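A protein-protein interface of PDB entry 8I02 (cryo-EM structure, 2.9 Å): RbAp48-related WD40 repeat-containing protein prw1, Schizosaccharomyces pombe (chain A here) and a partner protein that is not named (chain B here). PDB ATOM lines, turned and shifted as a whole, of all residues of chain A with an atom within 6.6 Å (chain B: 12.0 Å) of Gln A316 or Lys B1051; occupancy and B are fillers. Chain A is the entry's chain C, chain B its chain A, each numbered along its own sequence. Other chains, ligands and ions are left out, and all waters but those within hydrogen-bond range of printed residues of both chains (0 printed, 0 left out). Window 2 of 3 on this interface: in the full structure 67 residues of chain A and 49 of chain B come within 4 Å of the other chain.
The guanidinium group (NH2) of Arg A312 is in salt-bridge range of the side-chain carboxylate (OE2) of Glu B1047, at 3.2 Å. The side-chain amino group (NZ) of Lys B1051 sits close to the side-chain amide nitrogen (NE2) of Gln A316 (2.9 Å).
The backbone carbonyl oxygen (O) of Leu A308 lies within hydrogen-bond range of the backbone NH (N) of Leu A318, at 3.2 Å. The side-chain carboxylate (OD2) of Asp A310 is in salt-bridge range of the guanidinium group (NH2) of Arg A312. The side-chain amide oxygen of Asn A313 is in hydrogen-bond range of the side-chain amide nitrogen of Asn A315 (2.6 Å).
OD2 of Asp A310 touches OE2 of Glu B1047 (3.8 Å). Lys B1051 touches Asn A313 (NZ to O, 3.8 Å). Leu A318 touches Leu B1050 (O to CD2, 3.6 Å). CD2 of Leu A318 touches CE of Lys B1051, at 3.6 Å.
No residue of chain B comes within 4 Å of Trp A309. Of the printed residues of chain B, Asp A310 touches Glu B1047 (3.8 Å). Arg A312 touches just one residue of chain B: Glu B1047. Of chain B, only Lys B1051 (3.8 Å) comes within 4 Å of Asn A313. Of the printed residues of chain B, Gln A316 touches Lys B1051. Of chain B, only Leu B1050 (3.6 Å) and Lys B1051 (3.6 Å) come within 4 Å of Leu A318. Of the printed residues of chain A, Glu B1047 touches Asp A310 (3.8 Å) and Arg A312 (3.2 Å). Of the printed residues of chain A, Leu B1050 touches Leu A318. Of the printed residues of chain A, Lys B1051 touches Asn A313, Gln A316 and Leu A318. Val B1053 touches none of the printed residues of chain A. The nearest residue of chain B that does not touch Gln A316 is Val B1053 (4.02 Å).
Hydrophobic or aromatic side chains of chain A that line the printed part of chain B: Leu A318. Among the printed residues, 6 pairs touch across the chains. Among the printed residues, Asp or Glu carboxylates within 4 Å of a Lys or Arg side-chain nitrogen of the other chain: Arg A312 with Glu B1047 (3.2 Å).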
ATOM      1  N   VAL A 277     -11.891  -2.979  -9.151  1.00  0.00           N
ATOM      2  CA  VAL A 277     -10.751  -3.867  -8.939  1.00  0.00           C
ATOM      3  C   VAL A 277     -10.544  -4.132  -7.452  1.00  0.00           C
ATOM      4  O   VAL A 277     -10.548  -3.205  -6.633  1.00  0.00           O
ATOM      5  CB  VAL A 277      -9.489  -3.274  -9.581  1.00  0.00           C
ATOM      6  CG1 VAL A 277      -8.280  -4.127  -9.261  1.00  0.00           C
ATOM      7  CG2 VAL A 277      -9.676  -3.175 -11.078  1.00  0.00           C
ATOM      8  N   LEU A 308       0.721   1.106  -6.699  1.00  0.00           N
ATOM      9  CA  LEU A 308       0.554   2.024  -7.816  1.00  0.00           C
ATOM     10  C   LEU A 308      -0.051   1.291  -9.005  1.00  0.00           C
ATOM     11  O   LEU A 308       0.217   0.108  -9.224  1.00  0.00           O
ATOM     12  CB  LEU A 308       1.878   2.688  -8.195  1.00  0.00           C
ATOM     13  CG  LEU A 308       2.900   2.005  -9.089  1.00  0.00           C
ATOM     14  CD1 LEU A 308       2.672   2.397 -10.525  1.00  0.00           C
ATOM     15  CD2 LEU A 308       4.285   2.415  -8.657  1.00  0.00           C
ATOM     16  N   TRP A 309      -0.866   2.009  -9.770  1.00  0.00           N
ATOM     17  CA  TRP A 309      -1.831   1.417 -10.679  1.00  0.00           C
ATOM     18  C   TRP A 309      -1.758   2.087 -12.039  1.00  0.00           C
ATOM     19  O   TRP A 309      -1.335   3.237 -12.165  1.00  0.00           O
ATOM     20  CB  TRP A 309      -3.251   1.558 -10.127  1.00  0.00           C
ATOM     21  CG  TRP A 309      -3.744   0.344  -9.457  1.00  0.00           C
ATOM     22  CD1 TRP A 309      -4.055   0.196  -8.141  1.00  0.00           C
ATOM     23  CD2 TRP A 309      -3.982  -0.916 -10.075  1.00  0.00           C
ATOM     24  NE1 TRP A 309      -4.479  -1.089  -7.901  1.00  0.00           N
ATOM     25  CE2 TRP A 309      -4.442  -1.789  -9.077  1.00  0.00           C
ATOM     26  CE3 TRP A 309      -3.853  -1.393 -11.380  1.00  0.00           C
ATOM     27  CZ2 TRP A 309      -4.769  -3.108  -9.345  1.00  0.00           C
ATOM     28  CZ3 TRP A 309      -4.175  -2.701 -11.637  1.00  0.00           C
ATOM     29  CH2 TRP A 309      -4.632  -3.544 -10.627  1.00  0.00           C
ATOM     30  N   ASP A 310      -2.216   1.370 -13.056  1.00  0.00           N
ATOM     31  CA  ASP A 310      -2.298   1.907 -14.405  1.00  0.00           C
ATOM     32  C   ASP A 310      -3.692   1.646 -14.951  1.00  0.00           C
ATOM     33  O   ASP A 310      -4.246   0.560 -14.760  1.00  0.00           O
ATOM     34  CB  ASP A 310      -1.231   1.284 -15.316  1.00  0.00           C
ATOM     35  CG  ASP A 310      -0.693   2.262 -16.342  1.00  0.00           C
ATOM     36  OD1 ASP A 310      -1.499   3.007 -16.931  1.00  0.00           O
ATOM     37  OD2 ASP A 310       0.539   2.290 -16.554  1.00  0.00           O
ATOM     38  N   ARG A 312      -4.774   1.854 -18.240  1.00  0.00           N
ATOM     39  CA  ARG A 312      -4.892   1.170 -19.526  1.00  0.00           C
ATOM     40  C   ARG A 312      -5.240  -0.300 -19.336  1.00  0.00           C
ATOM     41  O   ARG A 312      -6.103  -0.839 -20.036  1.00  0.00           O
ATOM     42  CB  ARG A 312      -3.597   1.320 -20.322  1.00  0.00           C
ATOM     43  CG  ARG A 312      -3.379   2.705 -20.896  1.00  0.00           C
ATOM     44  CD  ARG A 312      -1.948   2.866 -21.369  1.00  0.00           C
ATOM     45  NE  ARG A 312      -1.007   2.732 -20.260  1.00  0.00           N
ATOM     46  CZ  ARG A 312       0.311   2.862 -20.371  1.00  0.00           C
ATOM     47  NH1 ARG A 312       0.857   3.136 -21.548  1.00  0.00           N
ATOM     48  NH2 ARG A 312       1.081   2.718 -19.305  1.00  0.00           N
ATOM     49  N   ASN A 313      -4.579  -0.964 -18.389  1.00  0.00           N
ATOM     50  CA  ASN A 313      -4.894  -2.343 -18.013  1.00  0.00           C
ATOM     51  C   ASN A 313      -4.839  -2.399 -16.492  1.00  0.00           C
ATOM     52  O   ASN A 313      -3.763  -2.545 -15.908  1.00  0.00           O
ATOM     53  CB  ASN A 313      -3.927  -3.338 -18.643  1.00  0.00           C
ATOM     54  CG  ASN A 313      -4.329  -4.782 -18.404  1.00  0.00           C
ATOM     55  OD1 ASN A 313      -5.073  -5.090 -17.472  1.00  0.00           O
ATOM     56  ND2 ASN A 313      -3.828  -5.680 -19.244  1.00  0.00           N
ATOM     57  N   LEU A 314      -6.000  -2.271 -15.856  1.00  0.00           N
ATOM     58  CA  LEU A 314      -6.085  -2.218 -14.399  1.00  0.00           C
ATOM     59  C   LEU A 314      -6.545  -3.574 -13.864  1.00  0.00           C
ATOM     60  O   LEU A 314      -7.687  -3.764 -13.445  1.00  0.00           O
ATOM     61  CB  LEU A 314      -6.985  -1.056 -13.974  1.00  0.00           C
ATOM     62  CG  LEU A 314      -8.470  -1.010 -14.334  1.00  0.00           C
ATOM     63  CD1 LEU A 314      -9.252  -0.355 -13.218  1.00  0.00           C
ATOM     64  CD2 LEU A 314      -8.683  -0.272 -15.645  1.00  0.00           C
ATOM     65  N   ASN A 315      -5.621  -4.530 -13.871  1.00  0.00           N
ATOM     66  CA  ASN A 315      -5.868  -5.854 -13.312  1.00  0.00           C
ATOM     67  C   ASN A 315      -4.796  -6.311 -12.337  1.00  0.00           C
ATOM     68  O   ASN A 315      -5.111  -6.993 -11.360  1.00  0.00           O
ATOM     69  CB  ASN A 315      -6.014  -6.892 -14.433  1.00  0.00           C
ATOM     70  CG  ASN A 315      -7.152  -6.570 -15.382  1.00  0.00           C
ATOM     71  OD1 ASN A 315      -8.238  -6.174 -14.957  1.00  0.00           O
ATOM     72  ND2 ASN A 315      -6.911  -6.751 -16.674  1.00  0.00           N
ATOM     73  N   GLN A 316      -3.535  -5.951 -12.564  1.00  0.00           N
ATOM     74  CA  GLN A 316      -2.455  -6.287 -11.647  1.00  0.00           C
ATOM     75  C   GLN A 316      -1.651  -5.035 -11.327  1.00  0.00           C
ATOM     76  O   GLN A 316      -1.400  -4.205 -12.203  1.00  0.00           O
ATOM     77  CB  GLN A 316      -1.541  -7.380 -12.223  1.00  0.00           C
ATOM     78  CG  GLN A 316      -0.781  -7.007 -13.491  1.00  0.00           C
ATOM     79  CD  GLN A 316      -1.680  -6.861 -14.703  1.00  0.00           C
ATOM     80  OE1 GLN A 316      -2.858  -7.210 -14.659  1.00  0.00           O
ATOM     81  NE2 GLN A 316      -1.127  -6.344 -15.792  1.00  0.00           N
ATOM     82  N   ARG A 317      -1.255  -4.903 -10.064  1.00  0.00           N
ATOM     83  CA  ARG A 317      -0.523  -3.726  -9.617  1.00  0.00           C
ATOM     84  C   ARG A 317       0.871  -3.683 -10.234  1.00  0.00           C
ATOM     85  O   ARG A 317       1.595  -4.681 -10.245  1.00  0.00           O
ATOM     86  CB  ARG A 317      -0.434  -3.723  -8.094  1.00  0.00           C
ATOM     87  CG  ARG A 317      -0.303  -5.115  -7.503  1.00  0.00           C
ATOM     88  CD  ARG A 317      -0.390  -5.108  -5.985  1.00  0.00           C
ATOM     89  NE  ARG A 317      -1.672  -4.612  -5.498  1.00  0.00           N
ATOM     90  CZ  ARG A 317      -2.014  -4.573  -4.215  1.00  0.00           C
ATOM     91  NH1 ARG A 317      -1.174  -5.005  -3.288  1.00  0.00           N
ATOM     92  NH2 ARG A 317      -3.197  -4.104  -3.858  1.00  0.00           N
ATOM     93  N   LEU A 318       1.250  -2.505 -10.735  1.00  0.00           N
ATOM     94  CA  LEU A 318       2.505  -2.369 -11.471  1.00  0.00           C
ATOM     95  C   LEU A 318       3.706  -2.690 -10.595  1.00  0.00           C
ATOM     96  O   LEU A 318       4.614  -3.415 -11.014  1.00  0.00           O
ATOM     97  CB  LEU A 318       2.633  -0.957 -12.034  1.00  0.00           C
ATOM     98  CG  LEU A 318       1.520  -0.473 -12.951  1.00  0.00           C
ATOM     99  CD1 LEU A 318       1.970   0.763 -13.697  1.00  0.00           C
ATOM    100  CD2 LEU A 318       1.134  -1.573 -13.907  1.00  0.00           C
ATOM    101  N   HIS A 319       3.745  -2.136  -9.386  1.00  0.00           N
ATOM    102  CA  HIS A 319       4.866  -2.378  -8.481  1.00  0.00           C
ATOM    103  C   HIS A 319       4.422  -2.025  -7.067  1.00  0.00           C
ATOM    104  O   HIS A 319       4.231  -0.848  -6.759  1.00  0.00           O
ATOM    105  CB  HIS A 319       6.079  -1.558  -8.899  1.00  0.00           C
ATOM    106  CG  HIS A 319       7.270  -1.753  -8.017  1.00  0.00           C
ATOM    107  ND1 HIS A 319       7.805  -2.994  -7.755  1.00  0.00           N
ATOM    108  CD2 HIS A 319       8.021  -0.867  -7.325  1.00  0.00           C
ATOM    109  CE1 HIS A 319       8.840  -2.864  -6.945  1.00  0.00           C
ATOM    110  NE2 HIS A 319       8.992  -1.582  -6.669  1.00  0.00           N
ATOM    111  N   TRP B1042      13.509   8.970 -17.433  1.00  0.00           N
ATOM    112  CA  TRP B1042      13.698   7.655 -16.833  1.00  0.00           C
ATOM    113  C   TRP B1042      12.373   7.048 -16.397  1.00  0.00           C
ATOM    114  O   TRP B1042      12.185   5.832 -16.496  1.00  0.00           O
ATOM    115  CB  TRP B1042      14.664   7.757 -15.653  1.00  0.00           C
ATOM    116  CG  TRP B1042      15.245   6.446 -15.226  1.00  0.00           C
ATOM    117  CD1 TRP B1042      15.106   5.245 -15.856  1.00  0.00           C
ATOM    118  CD2 TRP B1042      16.066   6.205 -14.077  1.00  0.00           C
ATOM    119  NE1 TRP B1042      15.784   4.269 -15.170  1.00  0.00           N
ATOM    120  CE2 TRP B1042      16.381   4.830 -14.073  1.00  0.00           C
ATOM    121  CE3 TRP B1042      16.564   7.015 -13.051  1.00  0.00           C
ATOM    122  CZ2 TRP B1042      17.170   4.248 -13.084  1.00  0.00           C
ATOM    123  CZ3 TRP B1042      17.343   6.436 -12.068  1.00  0.00           C
ATOM    124  CH2 TRP B1042      17.639   5.064 -12.093  1.00  0.00           C
ATOM    125  N   ARG B1043      11.428   7.879 -15.957  1.00  0.00           N
ATOM    126  CA  ARG B1043      10.145   7.360 -15.513  1.00  0.00           C
ATOM    127  C   ARG B1043       9.323   6.863 -16.687  1.00  0.00           C
ATOM    128  O   ARG B1043       8.664   5.826 -16.586  1.00  0.00           O
ATOM    129  CB  ARG B1043       9.380   8.430 -14.744  1.00  0.00           C
ATOM    130  CG  ARG B1043       8.310   7.875 -13.833  1.00  0.00           C
ATOM    131  CD  ARG B1043       6.985   7.703 -14.542  1.00  0.00           C
ATOM    132  NE  ARG B1043       5.957   7.189 -13.649  1.00  0.00           N
ATOM    133  CZ  ARG B1043       5.844   5.913 -13.296  1.00  0.00           C
ATOM    134  NH1 ARG B1043       6.706   5.017 -13.750  1.00  0.00           N
ATOM    135  NH2 ARG B1043       4.873   5.535 -12.482  1.00  0.00           N
ATOM    136  N   ASN B1044       9.334   7.587 -17.805  1.00  0.00           N
ATOM    137  CA  ASN B1044       8.633   7.094 -18.984  1.00  0.00           C
ATOM    138  C   ASN B1044       9.240   5.783 -19.462  1.00  0.00           C
ATOM    139  O   ASN B1044       8.513   4.850 -19.829  1.00  0.00           O
ATOM    140  CB  ASN B1044       8.657   8.143 -20.094  1.00  0.00           C
ATOM    141  CG  ASN B1044       7.627   9.231 -19.884  1.00  0.00           C
ATOM    142  OD1 ASN B1044       6.592   9.006 -19.265  1.00  0.00           O
ATOM    143  ND2 ASN B1044       7.905  10.418 -20.404  1.00  0.00           N
ATOM    144  N   ARG B1045      10.572   5.683 -19.439  1.00  0.00           N
ATOM    145  CA  ARG B1045      11.218   4.438 -19.841  1.00  0.00           C
ATOM    146  C   ARG B1045      10.790   3.281 -18.944  1.00  0.00           C
ATOM    147  O   ARG B1045      10.376   2.220 -19.431  1.00  0.00           O
ATOM    148  CB  ARG B1045      12.734   4.601 -19.815  1.00  0.00           C
ATOM    149  CG  ARG B1045      13.465   3.664 -20.753  1.00  0.00           C
ATOM    150  CD  ARG B1045      14.658   4.357 -21.371  1.00  0.00           C
ATOM    151  NE  ARG B1045      14.353   5.748 -21.695  1.00  0.00           N
ATOM    152  CZ  ARG B1045      13.715   6.139 -22.794  1.00  0.00           C
ATOM    153  NH1 ARG B1045      13.309   5.246 -23.686  1.00  0.00           N
ATOM    154  NH2 ARG B1045      13.483   7.428 -22.999  1.00  0.00           N
ATOM    155  N   TRP B1046      10.884   3.468 -17.626  1.00  0.00           N
ATOM    156  CA  TRP B1046      10.537   2.386 -16.716  1.00  0.00           C
ATOM    157  C   TRP B1046       9.045   2.084 -16.733  1.00  0.00           C
ATOM    158  O   TRP B1046       8.648   0.959 -16.420  1.00  0.00           O
ATOM    159  CB  TRP B1046      10.990   2.703 -15.293  1.00  0.00           C
ATOM    160  CG  TRP B1046      12.194   1.917 -14.871  1.00  0.00           C
ATOM    161  CD1 TRP B1046      13.355   2.416 -14.377  1.00  0.00           C
ATOM    162  CD2 TRP B1046      12.361   0.493 -14.932  1.00  0.00           C
ATOM    163  NE1 TRP B1046      14.235   1.399 -14.113  1.00  0.00           N
ATOM    164  CE2 TRP B1046      13.650   0.207 -14.447  1.00  0.00           C
ATOM    165  CE3 TRP B1046      11.547  -0.567 -15.343  1.00  0.00           C
ATOM    166  CZ2 TRP B1046      14.144  -1.092 -14.363  1.00  0.00           C
ATOM    167  CZ3 TRP B1046      12.042  -1.856 -15.259  1.00  0.00           C
ATOM    168  CH2 TRP B1046      13.326  -2.107 -14.773  1.00  0.00           C
ATOM    169  N   GLU B1047       8.203   3.058 -17.079  1.00  0.00           N
ATOM    170  CA  GLU B1047       6.777   2.778 -17.185  1.00  0.00           C
ATOM    171  C   GLU B1047       6.476   1.956 -18.429  1.00  0.00           C
ATOM    172  O   GLU B1047       5.681   1.009 -18.377  1.00  0.00           O
ATOM    173  CB  GLU B1047       5.979   4.082 -17.195  1.00  0.00           C
ATOM    174  CG  GLU B1047       4.486   3.896 -17.413  1.00  0.00           C
ATOM    175  CD  GLU B1047       3.751   5.208 -17.609  1.00  0.00           C
ATOM    176  OE1 GLU B1047       4.345   6.272 -17.348  1.00  0.00           O
ATOM    177  OE2 GLU B1047       2.573   5.178 -18.020  1.00  0.00           O
ATOM    178  N   SER B1048       7.106   2.298 -19.557  1.00  0.00           N
ATOM    179  CA  SER B1048       6.901   1.519 -20.772  1.00  0.00           C
ATOM    180  C   SER B1048       7.429   0.101 -20.611  1.00  0.00           C
ATOM    181  O   SER B1048       6.825  -0.855 -21.110  1.00  0.00           O
ATOM    182  CB  SER B1048       7.566   2.207 -21.962  1.00  0.00           C
ATOM    183  OG  SER B1048       7.450   3.613 -21.866  1.00  0.00           O
ATOM    184  N   LEU B1049       8.547  -0.061 -19.902  1.00  0.00           N
ATOM    185  CA  LEU B1049       9.092  -1.400 -19.697  1.00  0.00           C
ATOM    186  C   LEU B1049       8.264  -2.177 -18.680  1.00  0.00           C
ATOM    187  O   LEU B1049       7.954  -3.356 -18.883  1.00  0.00           O
ATOM    188  CB  LEU B1049      10.558  -1.319 -19.267  1.00  0.00           C
ATOM    189  CG  LEU B1049      11.561  -0.688 -20.239  1.00  0.00           C
ATOM    190  CD1 LEU B1049      12.922  -1.351 -20.091  1.00  0.00           C
ATOM    191  CD2 LEU B1049      11.085  -0.766 -21.688  1.00  0.00           C
ATOM    192  N   LEU B1050       7.901  -1.532 -17.572  1.00  0.00           N
ATOM    193  CA  LEU B1050       7.149  -2.189 -16.514  1.00  0.00           C
ATOM    194  C   LEU B1050       5.752  -2.592 -16.951  1.00  0.00           C
ATOM    195  O   LEU B1050       5.186  -3.530 -16.380  1.00  0.00           O
ATOM    196  CB  LEU B1050       7.054  -1.265 -15.299  1.00  0.00           C
ATOM    197  CG  LEU B1050       7.656  -1.752 -13.984  1.00  0.00           C
ATOM    198  CD1 LEU B1050       7.423  -0.725 -12.891  1.00  0.00           C
ATOM    199  CD2 LEU B1050       7.060  -3.095 -13.605  1.00  0.00           C
ATOM    200  N   LYS B1051       5.179  -1.907 -17.938  1.00  0.00           N
ATOM    201  CA  LYS B1051       3.883  -2.296 -18.489  1.00  0.00           C
ATOM    202  C   LYS B1051       4.078  -3.083 -19.785  1.00  0.00           C
ATOM    203  O   LYS B1051       3.728  -2.662 -20.886  1.00  0.00           O
ATOM    204  CB  LYS B1051       2.994  -1.070 -18.685  1.00  0.00           C
ATOM    205  CG  LYS B1051       1.559  -1.332 -19.204  1.00  0.00           C
ATOM    206  CD  LYS B1051       0.922  -2.653 -18.742  1.00  0.00           C
ATOM    207  CE  LYS B1051       0.804  -2.783 -17.229  1.00  0.00           C
ATOM    208  NZ  LYS B1051      -0.279  -3.717 -16.827  1.00  0.00           N
ATOM    209  N   SER B1052       4.691  -4.249 -19.622  1.00  0.00           N
ATOM    210  CA  SER B1052       4.699  -5.268 -20.657  1.00  0.00           C
ATOM    211  C   SER B1052       4.470  -6.654 -20.081  1.00  0.00           C
ATOM    212  O   SER B1052       4.510  -7.632 -20.832  1.00  0.00           O
ATOM    213  CB  SER B1052       6.020  -5.245 -21.445  1.00  0.00           C
ATOM    214  OG  SER B1052       6.898  -6.262 -21.001  1.00  0.00           O
ATOM    215  N   VAL B1053       4.229  -6.767 -18.780  1.00  0.00           N
ATOM    216  CA  VAL B1053       3.922  -8.040 -18.157  1.00  0.00           C
ATOM    217  C   VAL B1053       2.417  -8.250 -18.204  1.00  0.00           C
ATOM    218  O   VAL B1053       1.668  -7.324 -18.516  1.00  0.00           O
ATOM    219  CB  VAL B1053       4.441  -8.097 -16.714  1.00  0.00           C
ATOM    220  CG1 VAL B1053       5.880  -7.600 -16.650  1.00  0.00           C
ATOM    221  CG2 VAL B1053       3.541  -7.286 -15.796  1.00  0.00           C
